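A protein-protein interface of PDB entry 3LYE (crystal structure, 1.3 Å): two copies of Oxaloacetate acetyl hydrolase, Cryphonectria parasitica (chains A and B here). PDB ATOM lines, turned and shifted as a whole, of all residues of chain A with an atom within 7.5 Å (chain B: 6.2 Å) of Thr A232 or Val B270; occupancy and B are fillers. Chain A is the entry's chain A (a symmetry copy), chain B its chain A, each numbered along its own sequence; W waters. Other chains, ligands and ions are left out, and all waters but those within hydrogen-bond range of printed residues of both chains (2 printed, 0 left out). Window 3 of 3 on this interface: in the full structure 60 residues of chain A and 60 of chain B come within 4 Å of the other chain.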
ATOM      1  N   LEU A  26      24.199  13.164   2.329  1.00  0.00           N
ATOM      2  CA  LEU A  26      23.520  13.657   3.531  1.00  0.00           C
ATOM      3  C   LEU A  26      22.059  13.630   3.092  1.00  0.00           C
ATOM      4  O   LEU A  26      21.673  14.324   2.165  1.00  0.00           O
ATOM      5  CB  LEU A  26      23.938  15.083   3.901  1.00  0.00           C
ATOM      6  CG  LEU A  26      23.110  15.652   5.061  1.00  0.00           C
ATOM      7  CD1 LEU A  26      23.272  14.789   6.294  1.00  0.00           C
ATOM      8  CD2 LEU A  26      23.478  17.069   5.344  1.00  0.00           C
ATOM      9  N   LYS A 203      28.686  23.661  17.366  1.00  0.00           N
ATOM     10  CA  LYS A 203      29.063  22.933  16.162  1.00  0.00           C
ATOM     11  C   LYS A 203      30.238  21.996  16.459  1.00  0.00           C
ATOM     12  O   LYS A 203      30.325  20.905  15.900  1.00  0.00           O
ATOM     13  CB  LYS A 203      29.429  23.903  15.053  1.00  0.00           C
ATOM     14  CG  LYS A 203      28.285  24.831  14.696  1.00  0.00           C
ATOM     15  CD  LYS A 203      28.733  25.929  13.773  1.00  0.00           C
ATOM     16  CE  LYS A 203      29.354  25.404  12.504  1.00  0.00           C
ATOM     17  NZ  LYS A 203      29.915  26.534  11.724  1.00  0.00           N
ATOM     18  N   LEU A 220      21.289  14.501  12.427  1.00  0.00           N
ATOM     19  CA  LEU A 220      21.294  15.830  13.016  1.00  0.00           C
ATOM     20  C   LEU A 220      19.879  16.403  12.949  1.00  0.00           C
ATOM     21  O   LEU A 220      19.302  16.485  11.882  1.00  0.00           O
ATOM     22  CB  LEU A 220      22.234  16.761  12.232  1.00  0.00           C
ATOM     23  CG  LEU A 220      22.292  18.206  12.696  1.00  0.00           C
ATOM     24  CD1 LEU A 220      22.769  18.316  14.124  1.00  0.00           C
ATOM     25  CD2 LEU A 220      23.170  19.011  11.786  1.00  0.00           C
ATOM     26  N   SER A 222      17.786  19.586  13.184  1.00  0.00           N
ATOM     27  CA  SER A 222      17.804  21.046  13.120  1.00  0.00           C
ATOM     28  C   SER A 222      16.419  21.572  13.546  1.00  0.00           C
ATOM     29  O   SER A 222      15.443  21.294  12.902  1.00  0.00           O
ATOM     30  CB  SER A 222      18.115  21.453  11.689  1.00  0.00           C
ATOM     31  OG  SER A 222      18.250  22.852  11.586  1.00  0.00           O
ATOM     32  N   GLU A 224      14.241  24.707  13.831  1.00  0.00           N
ATOM     33  CA  GLU A 224      14.201  26.102  13.418  1.00  0.00           C
ATOM     34  C   GLU A 224      13.737  27.017  14.548  1.00  0.00           C
ATOM     35  O   GLU A 224      12.703  26.806  15.180  1.00  0.00           O
ATOM     36  CB  GLU A 224      13.320  26.243  12.181  1.00  0.00           C
ATOM     37  CG  GLU A 224      13.172  27.679  11.674  1.00  0.00           C
ATOM     38  CD  GLU A 224      14.499  28.304  11.180  1.00  0.00           C
ATOM     39  OE1 GLU A 224      14.525  29.540  10.953  1.00  0.00           O
ATOM     40  OE2 GLU A 224      15.517  27.592  11.031  1.00  0.00           O
ATOM     41  N   PRO A 229      22.627  25.836  17.881  1.00  0.00           N
ATOM     42  CA  PRO A 229      23.208  26.707  16.858  1.00  0.00           C
ATOM     43  C   PRO A 229      22.805  26.328  15.441  1.00  0.00           C
ATOM     44  O   PRO A 229      22.481  25.177  15.141  1.00  0.00           O
ATOM     45  CB  PRO A 229      24.712  26.511  17.046  1.00  0.00           C
ATOM     46  CG  PRO A 229      24.828  25.179  17.678  1.00  0.00           C
ATOM     47  CD  PRO A 229      23.673  25.073  18.593  1.00  0.00           C
ATOM     48  N   LEU A 230      22.878  27.308  14.555  1.00  0.00           N
ATOM     49  CA  LEU A 230      22.532  27.090  13.173  1.00  0.00           C
ATOM     50  C   LEU A 230      23.639  26.342  12.460  1.00  0.00           C
ATOM     51  O   LEU A 230      24.807  26.695  12.569  1.00  0.00           O
ATOM     52  CB  LEU A 230      22.337  28.432  12.480  1.00  0.00           C
ATOM     53  CG  LEU A 230      21.878  28.460  11.015  1.00  0.00           C
ATOM     54  CD1 LEU A 230      20.551  27.779  10.824  1.00  0.00           C
ATOM     55  CD2 LEU A 230      21.771  29.899  10.545  1.00  0.00           C
ATOM     56  N   ILE A 231      23.266  25.250  11.806  1.00  0.00           N
ATOM     57  CA  ILE A 231      24.194  24.434  11.048  1.00  0.00           C
ATOM     58  C   ILE A 231      23.576  24.284   9.648  1.00  0.00           C
ATOM     59  O   ILE A 231      22.421  23.892   9.516  1.00  0.00           O
ATOM     60  CB  ILE A 231      24.408  23.049  11.682  1.00  0.00           C
ATOM     61  CG1 ILE A 231      25.045  23.203  13.071  1.00  0.00           C
ATOM     62  CG2 ILE A 231      25.280  22.207  10.781  1.00  0.00           C
ATOM     63  CD1 ILE A 231      25.167  21.944  13.895  1.00  0.00           C
ATOM     64  N   THR A 232      24.307  24.664   8.603  1.00  0.00           N
ATOM     65  CA  THR A 232      23.755  24.529   7.258  1.00  0.00           C
ATOM     66  C   THR A 232      23.892  23.100   6.763  1.00  0.00           C
ATOM     67  O   THR A 232      24.591  22.289   7.352  1.00  0.00           O
ATOM     68  CB  THR A 232      24.469  25.426   6.237  1.00  0.00           C
ATOM     69  OG1 THR A 232      25.815  24.960   6.055  1.00  0.00           O
ATOM     70  CG2 THR A 232      24.528  26.867   6.719  1.00  0.00           C
ATOM     71  N   VAL A 233      23.198  22.799   5.671  1.00  0.00           N
ATOM     72  CA  VAL A 233      23.259  21.473   5.086  1.00  0.00           C
ATOM     73  C   VAL A 233      24.719  21.183   4.690  1.00  0.00           C
ATOM     74  O   VAL A 233      25.237  20.110   4.975  1.00  0.00           O
ATOM     75  CB  VAL A 233      22.320  21.388   3.881  1.00  0.00           C
ATOM     76  CG1 VAL A 233      22.641  20.187   3.003  1.00  0.00           C
ATOM     77  CG2 VAL A 233      20.850  21.393   4.346  1.00  0.00           C
ATOM     78  N   GLU A 234      25.393  22.145   4.064  1.00  0.00           N
ATOM     79  CA  GLU A 234      26.786  21.924   3.667  1.00  0.00           C
ATOM     80  C   GLU A 234      27.671  21.637   4.863  1.00  0.00           C
ATOM     81  O   GLU A 234      28.539  20.779   4.789  1.00  0.00           O
ATOM     82  CB  GLU A 234      27.314  23.142   2.923  1.00  0.00           C
ATOM     83  CG  GLU A 234      26.722  23.273   1.541  1.00  0.00           C
ATOM     84  CD  GLU A 234      27.333  24.422   0.750  1.00  0.00           C
ATOM     85  OE1 GLU A 234      28.429  24.908   1.131  1.00  0.00           O
ATOM     86  OE2 GLU A 234      26.712  24.839  -0.254  1.00  0.00           O
ATOM     87  N   GLU A 235      27.480  22.375   5.949  1.00  0.00           N
ATOM     88  CA  GLU A 235      28.264  22.174   7.157  1.00  0.00           C
ATOM     89  C   GLU A 235      28.009  20.796   7.783  1.00  0.00           C
ATOM     90  O   GLU A 235      28.951  20.113   8.204  1.00  0.00           O
ATOM     91  CB  GLU A 235      27.966  23.263   8.183  1.00  0.00           C
ATOM     92  CG  GLU A 235      28.566  24.629   7.843  1.00  0.00           C
ATOM     93  CD  GLU A 235      28.092  25.726   8.767  1.00  0.00           C
ATOM     94  OE1 GLU A 235      26.990  25.611   9.332  1.00  0.00           O
ATOM     95  OE2 GLU A 235      28.816  26.733   8.913  1.00  0.00           O
ATOM     96  N   ALA A 236      26.744  20.392   7.869  1.00  0.00           N
ATOM     97  CA  ALA A 236      26.416  19.092   8.451  1.00  0.00           C
ATOM     98  C   ALA A 236      27.037  17.977   7.624  1.00  0.00           C
ATOM     99  O   ALA A 236      27.518  17.000   8.156  1.00  0.00           O
ATOM    100  CB  ALA A 236      24.907  18.924   8.590  1.00  0.00           C
ATOM    101  N   LYS A 237      27.050  18.140   6.313  1.00  0.00           N
ATOM    102  CA  LYS A 237      27.621  17.130   5.427  1.00  0.00           C
ATOM    103  C   LYS A 237      29.120  17.009   5.671  1.00  0.00           C
ATOM    104  O   LYS A 237      29.689  15.909   5.735  1.00  0.00           O
ATOM    105  CB  LYS A 237      27.311  17.523   3.984  1.00  0.00           C
ATOM    106  CG  LYS A 237      28.101  16.791   2.935  1.00  0.00           C
ATOM    107  CD  LYS A 237      27.514  15.435   2.689  1.00  0.00           C
ATOM    108  CE  LYS A 237      28.355  14.635   1.701  1.00  0.00           C
ATOM    109  NZ  LYS A 237      27.864  14.859   0.309  1.00  0.00           N
ATOM    110  N   ALA A 238      29.778  18.155   5.800  1.00  0.00           N
ATOM    111  CA  ALA A 238      31.216  18.140   6.042  1.00  0.00           C
ATOM    112  C   ALA A 238      31.567  17.540   7.423  1.00  0.00           C
ATOM    113  O   ALA A 238      32.619  16.901   7.583  1.00  0.00           O
ATOM    114  CB  ALA A 238      31.785  19.536   5.867  1.00  0.00           C
ATOM    115  N   MET A 239      30.667  17.726   8.397  1.00  0.00           N
ATOM    116  CA  MET A 239      30.842  17.200   9.766  1.00  0.00           C
ATOM    117  C   MET A 239      30.731  15.671   9.754  1.00  0.00           C
ATOM    118  O   MET A 239      31.162  15.015  10.701  1.00  0.00           O
ATOM    119  CB  MET A 239      29.728  17.705  10.709  1.00  0.00           C
ATOM    120  CG  MET A 239      29.953  19.113  11.290  1.00  0.00           C
ATOM    121  SD  MET A 239      28.593  19.656  12.371  1.00  0.00           S
ATOM    122  CE  MET A 239      27.124  19.491  11.382  1.00  0.00           C
ATOM    123  N   MET A 244      19.759  14.564   8.068  1.00  0.00           N
ATOM    124  CA  MET A 244      19.524  15.840   8.732  1.00  0.00           C
ATOM    125  C   MET A 244      18.025  16.091   8.566  1.00  0.00           C
ATOM    126  O   MET A 244      17.506  16.106   7.452  1.00  0.00           O
ATOM    127  CB  MET A 244      20.328  16.969   8.117  1.00  0.00           C
ATOM    128  CG  MET A 244      20.207  18.273   8.840  1.00  0.00           C
ATOM    129  SD  MET A 244      21.426  19.417   8.177  1.00  0.00           S
ATOM    130  CE  MET A 244      21.160  20.883   9.172  1.00  0.00           C
ATOM    131  N   PHE A 246      14.604  18.496   9.617  1.00  0.00           N
ATOM    132  CA  PHE A 246      14.299  19.874   9.895  1.00  0.00           C
ATOM    133  C   PHE A 246      12.967  20.095  10.612  1.00  0.00           C
ATOM    134  O   PHE A 246      11.924  20.292   9.975  1.00  0.00           O
ATOM    135  CB  PHE A 246      14.372  20.621   8.557  1.00  0.00           C
ATOM    136  CG  PHE A 246      15.758  20.726   8.015  1.00  0.00           C
ATOM    137  CD1 PHE A 246      16.527  21.845   8.243  1.00  0.00           C
ATOM    138  CD2 PHE A 246      16.300  19.694   7.284  1.00  0.00           C
ATOM    139  CE1 PHE A 246      17.815  21.918   7.758  1.00  0.00           C
ATOM    140  CE2 PHE A 246      17.602  19.761   6.826  1.00  0.00           C
ATOM    141  CZ  PHE A 246      18.360  20.879   7.050  1.00  0.00           C
ATOM    142  N   THR B 261       9.599  28.449   1.628  1.00  0.00           N
ATOM    143  CA  THR B 261      10.574  28.032   2.623  1.00  0.00           C
ATOM    144  C   THR B 261      11.317  26.786   2.194  1.00  0.00           C
ATOM    145  O   THR B 261      12.536  26.668   2.316  1.00  0.00           O
ATOM    146  CB  THR B 261       9.911  27.807   3.972  1.00  0.00           C
ATOM    147  OG1 THR B 261       9.379  29.047   4.446  1.00  0.00           O
ATOM    148  CG2 THR B 261      10.892  27.267   4.979  1.00  0.00           C
ATOM    149  N   ARG B 264      13.876  27.421  -0.420  1.00  0.00           N
ATOM    150  CA  ARG B 264      15.074  27.981   0.216  1.00  0.00           C
ATOM    151  C   ARG B 264      15.888  26.849   0.843  1.00  0.00           C
ATOM    152  O   ARG B 264      17.102  26.832   0.734  1.00  0.00           O
ATOM    153  CB  ARG B 264      14.693  29.012   1.283  1.00  0.00           C
ATOM    154  CG  ARG B 264      15.859  29.736   1.914  1.00  0.00           C
ATOM    155  CD  ARG B 264      15.376  30.630   3.033  1.00  0.00           C
ATOM    156  NE  ARG B 264      14.399  31.570   2.505  1.00  0.00           N
ATOM    157  CZ  ARG B 264      13.140  31.746   2.915  1.00  0.00           C
ATOM    158  NH1 ARG B 264      12.600  31.123   3.958  1.00  0.00           N
ATOM    159  NH2 ARG B 264      12.425  32.630   2.265  1.00  0.00           N
ATOM    160  N   LEU B 265      15.248  25.908   1.527  1.00  0.00           N
ATOM    161  CA  LEU B 265      15.996  24.817   2.120  1.00  0.00           C
ATOM    162  C   LEU B 265      16.659  23.975   1.036  1.00  0.00           C
ATOM    163  O   LEU B 265      17.836  23.622   1.125  1.00  0.00           O
ATOM    164  CB  LEU B 265      15.066  23.928   2.949  1.00  0.00           C
ATOM    165  CG  LEU B 265      15.696  22.662   3.524  1.00  0.00           C
ATOM    166  CD1 LEU B 265      16.838  23.038   4.427  1.00  0.00           C
ATOM    167  CD2 LEU B 265      14.626  21.899   4.237  1.00  0.00           C
ATOM    168  N   ARG B 266      15.932  23.698  -0.023  1.00  0.00           N
ATOM    169  CA  ARG B 266      16.472  22.883  -1.089  1.00  0.00           C
ATOM    170  C   ARG B 266      17.663  23.501  -1.806  1.00  0.00           C
ATOM    171  O   ARG B 266      18.664  22.836  -2.057  1.00  0.00           O
ATOM    172  CB  ARG B 266      15.369  22.630  -2.150  1.00  0.00           C
ATOM    173  CG  ARG B 266      15.789  21.650  -3.264  1.00  0.00           C
ATOM    174  CD  ARG B 266      14.748  21.526  -4.365  1.00  0.00           C
ATOM    175  NE  ARG B 266      14.661  22.797  -5.064  1.00  0.00           N
ATOM    176  CZ  ARG B 266      13.653  23.194  -5.836  1.00  0.00           C
ATOM    177  NH1 ARG B 266      12.593  22.404  -6.053  1.00  0.00           N
ATOM    178  NH2 ARG B 266      13.727  24.391  -6.394  1.00  0.00           N
ATOM    179  N   HIS B 268      19.406  26.524  -0.801  1.00  0.00           N
ATOM    180  CA  HIS B 268      20.345  27.255   0.036  1.00  0.00           C
ATOM    181  C   HIS B 268      20.756  26.546   1.307  1.00  0.00           C
ATOM    182  O   HIS B 268      21.645  27.036   1.997  1.00  0.00           O
ATOM    183  CB  HIS B 268      19.828  28.664   0.312  1.00  0.00           C
ATOM    184  CG  HIS B 268      19.623  29.466  -0.931  1.00  0.00           C
ATOM    185  ND1 HIS B 268      20.666  29.999  -1.649  1.00  0.00           N
ATOM    186  CD2 HIS B 268      18.499  29.777  -1.614  1.00  0.00           C
ATOM    187  CE1 HIS B 268      20.190  30.624  -2.709  1.00  0.00           C
ATOM    188  NE2 HIS B 268      18.877  30.502  -2.712  1.00  0.00           N
ATOM    189  N   GLY B 269      20.075  25.454   1.665  1.00  0.00           N
ATOM    190  CA  GLY B 269      20.486  24.722   2.843  1.00  0.00           C
ATOM    191  C   GLY B 269      20.114  25.245   4.198  1.00  0.00           C
ATOM    192  O   GLY B 269      20.693  24.802   5.192  1.00  0.00           O
ATOM    193  N   VAL B 270      19.198  26.206   4.221  1.00  0.00           N
ATOM    194  CA  VAL B 270      18.704  26.799   5.446  1.00  0.00           C
ATOM    195  C   VAL B 270      17.200  27.043   5.284  1.00  0.00           C
ATOM    196  O   VAL B 270      16.695  27.296   4.194  1.00  0.00           O
ATOM    197  CB  VAL B 270      19.374  28.121   5.830  1.00  0.00           C
ATOM    198  CG1 VAL B 270      20.860  27.906   6.043  1.00  0.00           C
ATOM    199  CG2 VAL B 270      19.111  29.162   4.769  1.00  0.00           C
ATOM    200  N   VAL B 271      16.491  26.942   6.391  1.00  0.00           N
ATOM    201  CA  VAL B 271      15.026  27.153   6.433  1.00  0.00           C
ATOM    202  C   VAL B 271      14.754  28.649   6.398  1.00  0.00           C
ATOM    203  O   VAL B 271      13.900  29.126   5.653  1.00  0.00           O
ATOM    204  CB  VAL B 271      14.448  26.464   7.650  1.00  0.00           C
ATOM    205  CG1 VAL B 271      12.977  26.803   7.872  1.00  0.00           C
ATOM    206  CG2 VAL B 271      14.620  24.940   7.504  1.00  0.00           C
ATOM    207  N   GLY B 272      15.455  29.417   7.218  1.00  0.00           N
ATOM    208  CA  GLY B 272      15.281  30.860   7.195  1.00  0.00           C
ATOM    209  C   GLY B 272      14.012  31.540   7.636  1.00  0.00           C
ATOM    210  O   GLY B 272      13.665  32.623   7.134  1.00  0.00           O
HETATM  211  O   HOH W   1      20.190  24.477   7.936  1.00  0.00           O
HETATM  212  O   HOH W   2      17.408  28.579   9.375  1.00  0.00           O
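Water W2 lies within hydrogen-bond range of the side-chain carboxylate (OE2) of Glu A224 (2.7 Å) and the backbone NH (N) of Gly B272 (3.0 Å).
Water W1 lies within hydrogen-bond range of the backbone carbonyl oxygen (O) of Ile A231 and the backbone carbonyl oxygen (O) of Gly B269.
Printed residues of chain B that touch a printed residue of chain A: Leu B265, Gly B269, Val B270, Val B271 and Gly B272.
Hydrophobic or aromatic side chains of chain B that line the printed part of chain A: Leu B265, Val B270 and Val B271.
Of the 18 printed residues of chain A, 4 touch a printed residue of chain B.
Thr A232 touches just these residues of chain B: Gly B269 and Val B270.
Val B270 touches one residue of chain A.
Gly B269 touches just these residues of chain A: Thr A232 and Val A233.
Of the printed residues of chain A, Gly B272 touches Glu A224 (3.9 Å).
Printed residues of chain B within 4 Å of Phe A246: Leu B265 and Val B271.
Printed residues of chain B within 4 Å of Val A233: Gly B269.
Printed residues of chain A within 4 Å of Leu B265: Phe A246.
Of the printed residues of chain A, Val B271 touches Glu A224 (3.7 Å) and Phe A246 (3.7 Å).
The nearest printed residue of chain A that does not touch Gly B272 is Leu A230 (6.5 Å).
The backbone carbonyl oxygen (O) of Gly B269 lies within hydrogen-bond range of the backbone NH (N) of Val A233 (3.2 Å).
The backbone NH (N) of Leu B265 lies close to the backbone carbonyl oxygen (O) of Val B270 (3.3 Å).
The side-chain hydroxyl (OG1) of Thr A232 lies close to the backbone NH (N) of Glu A234 (3.5 Å).
The backbone carbonyl oxygen of Arg B264 is in hydrogen-bond range of the backbone NH of Gly B269, 3.4 Å away.
N of Thr A232 sits at hydrogen-bond distance from OE1 of Glu A235 (2.9 Å).
The guanidinium group (NH1) of Arg B264 is in hydrogen-bond range of the backbone carbonyl oxygen (O) of Val B271 (2.9 Å).
No position is printed for both chains.
Of the 7 pairs that touch across the chains among the printed residues, none has its exchanged pair printed and touching as well.
Among the printed residues, pairs that only touch across the chains: Glu A224 with Val B271 (3.7 Å), Glu A224 with Gly B272 (3.9 Å), Thr A232 with Gly B269 (3.7 Å), Thr A232 with Val B270 (3.9 Å), Phe A246 with Leu B265 (3.6 Å) and Phe A246 with Val B271 (3.7 Å).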
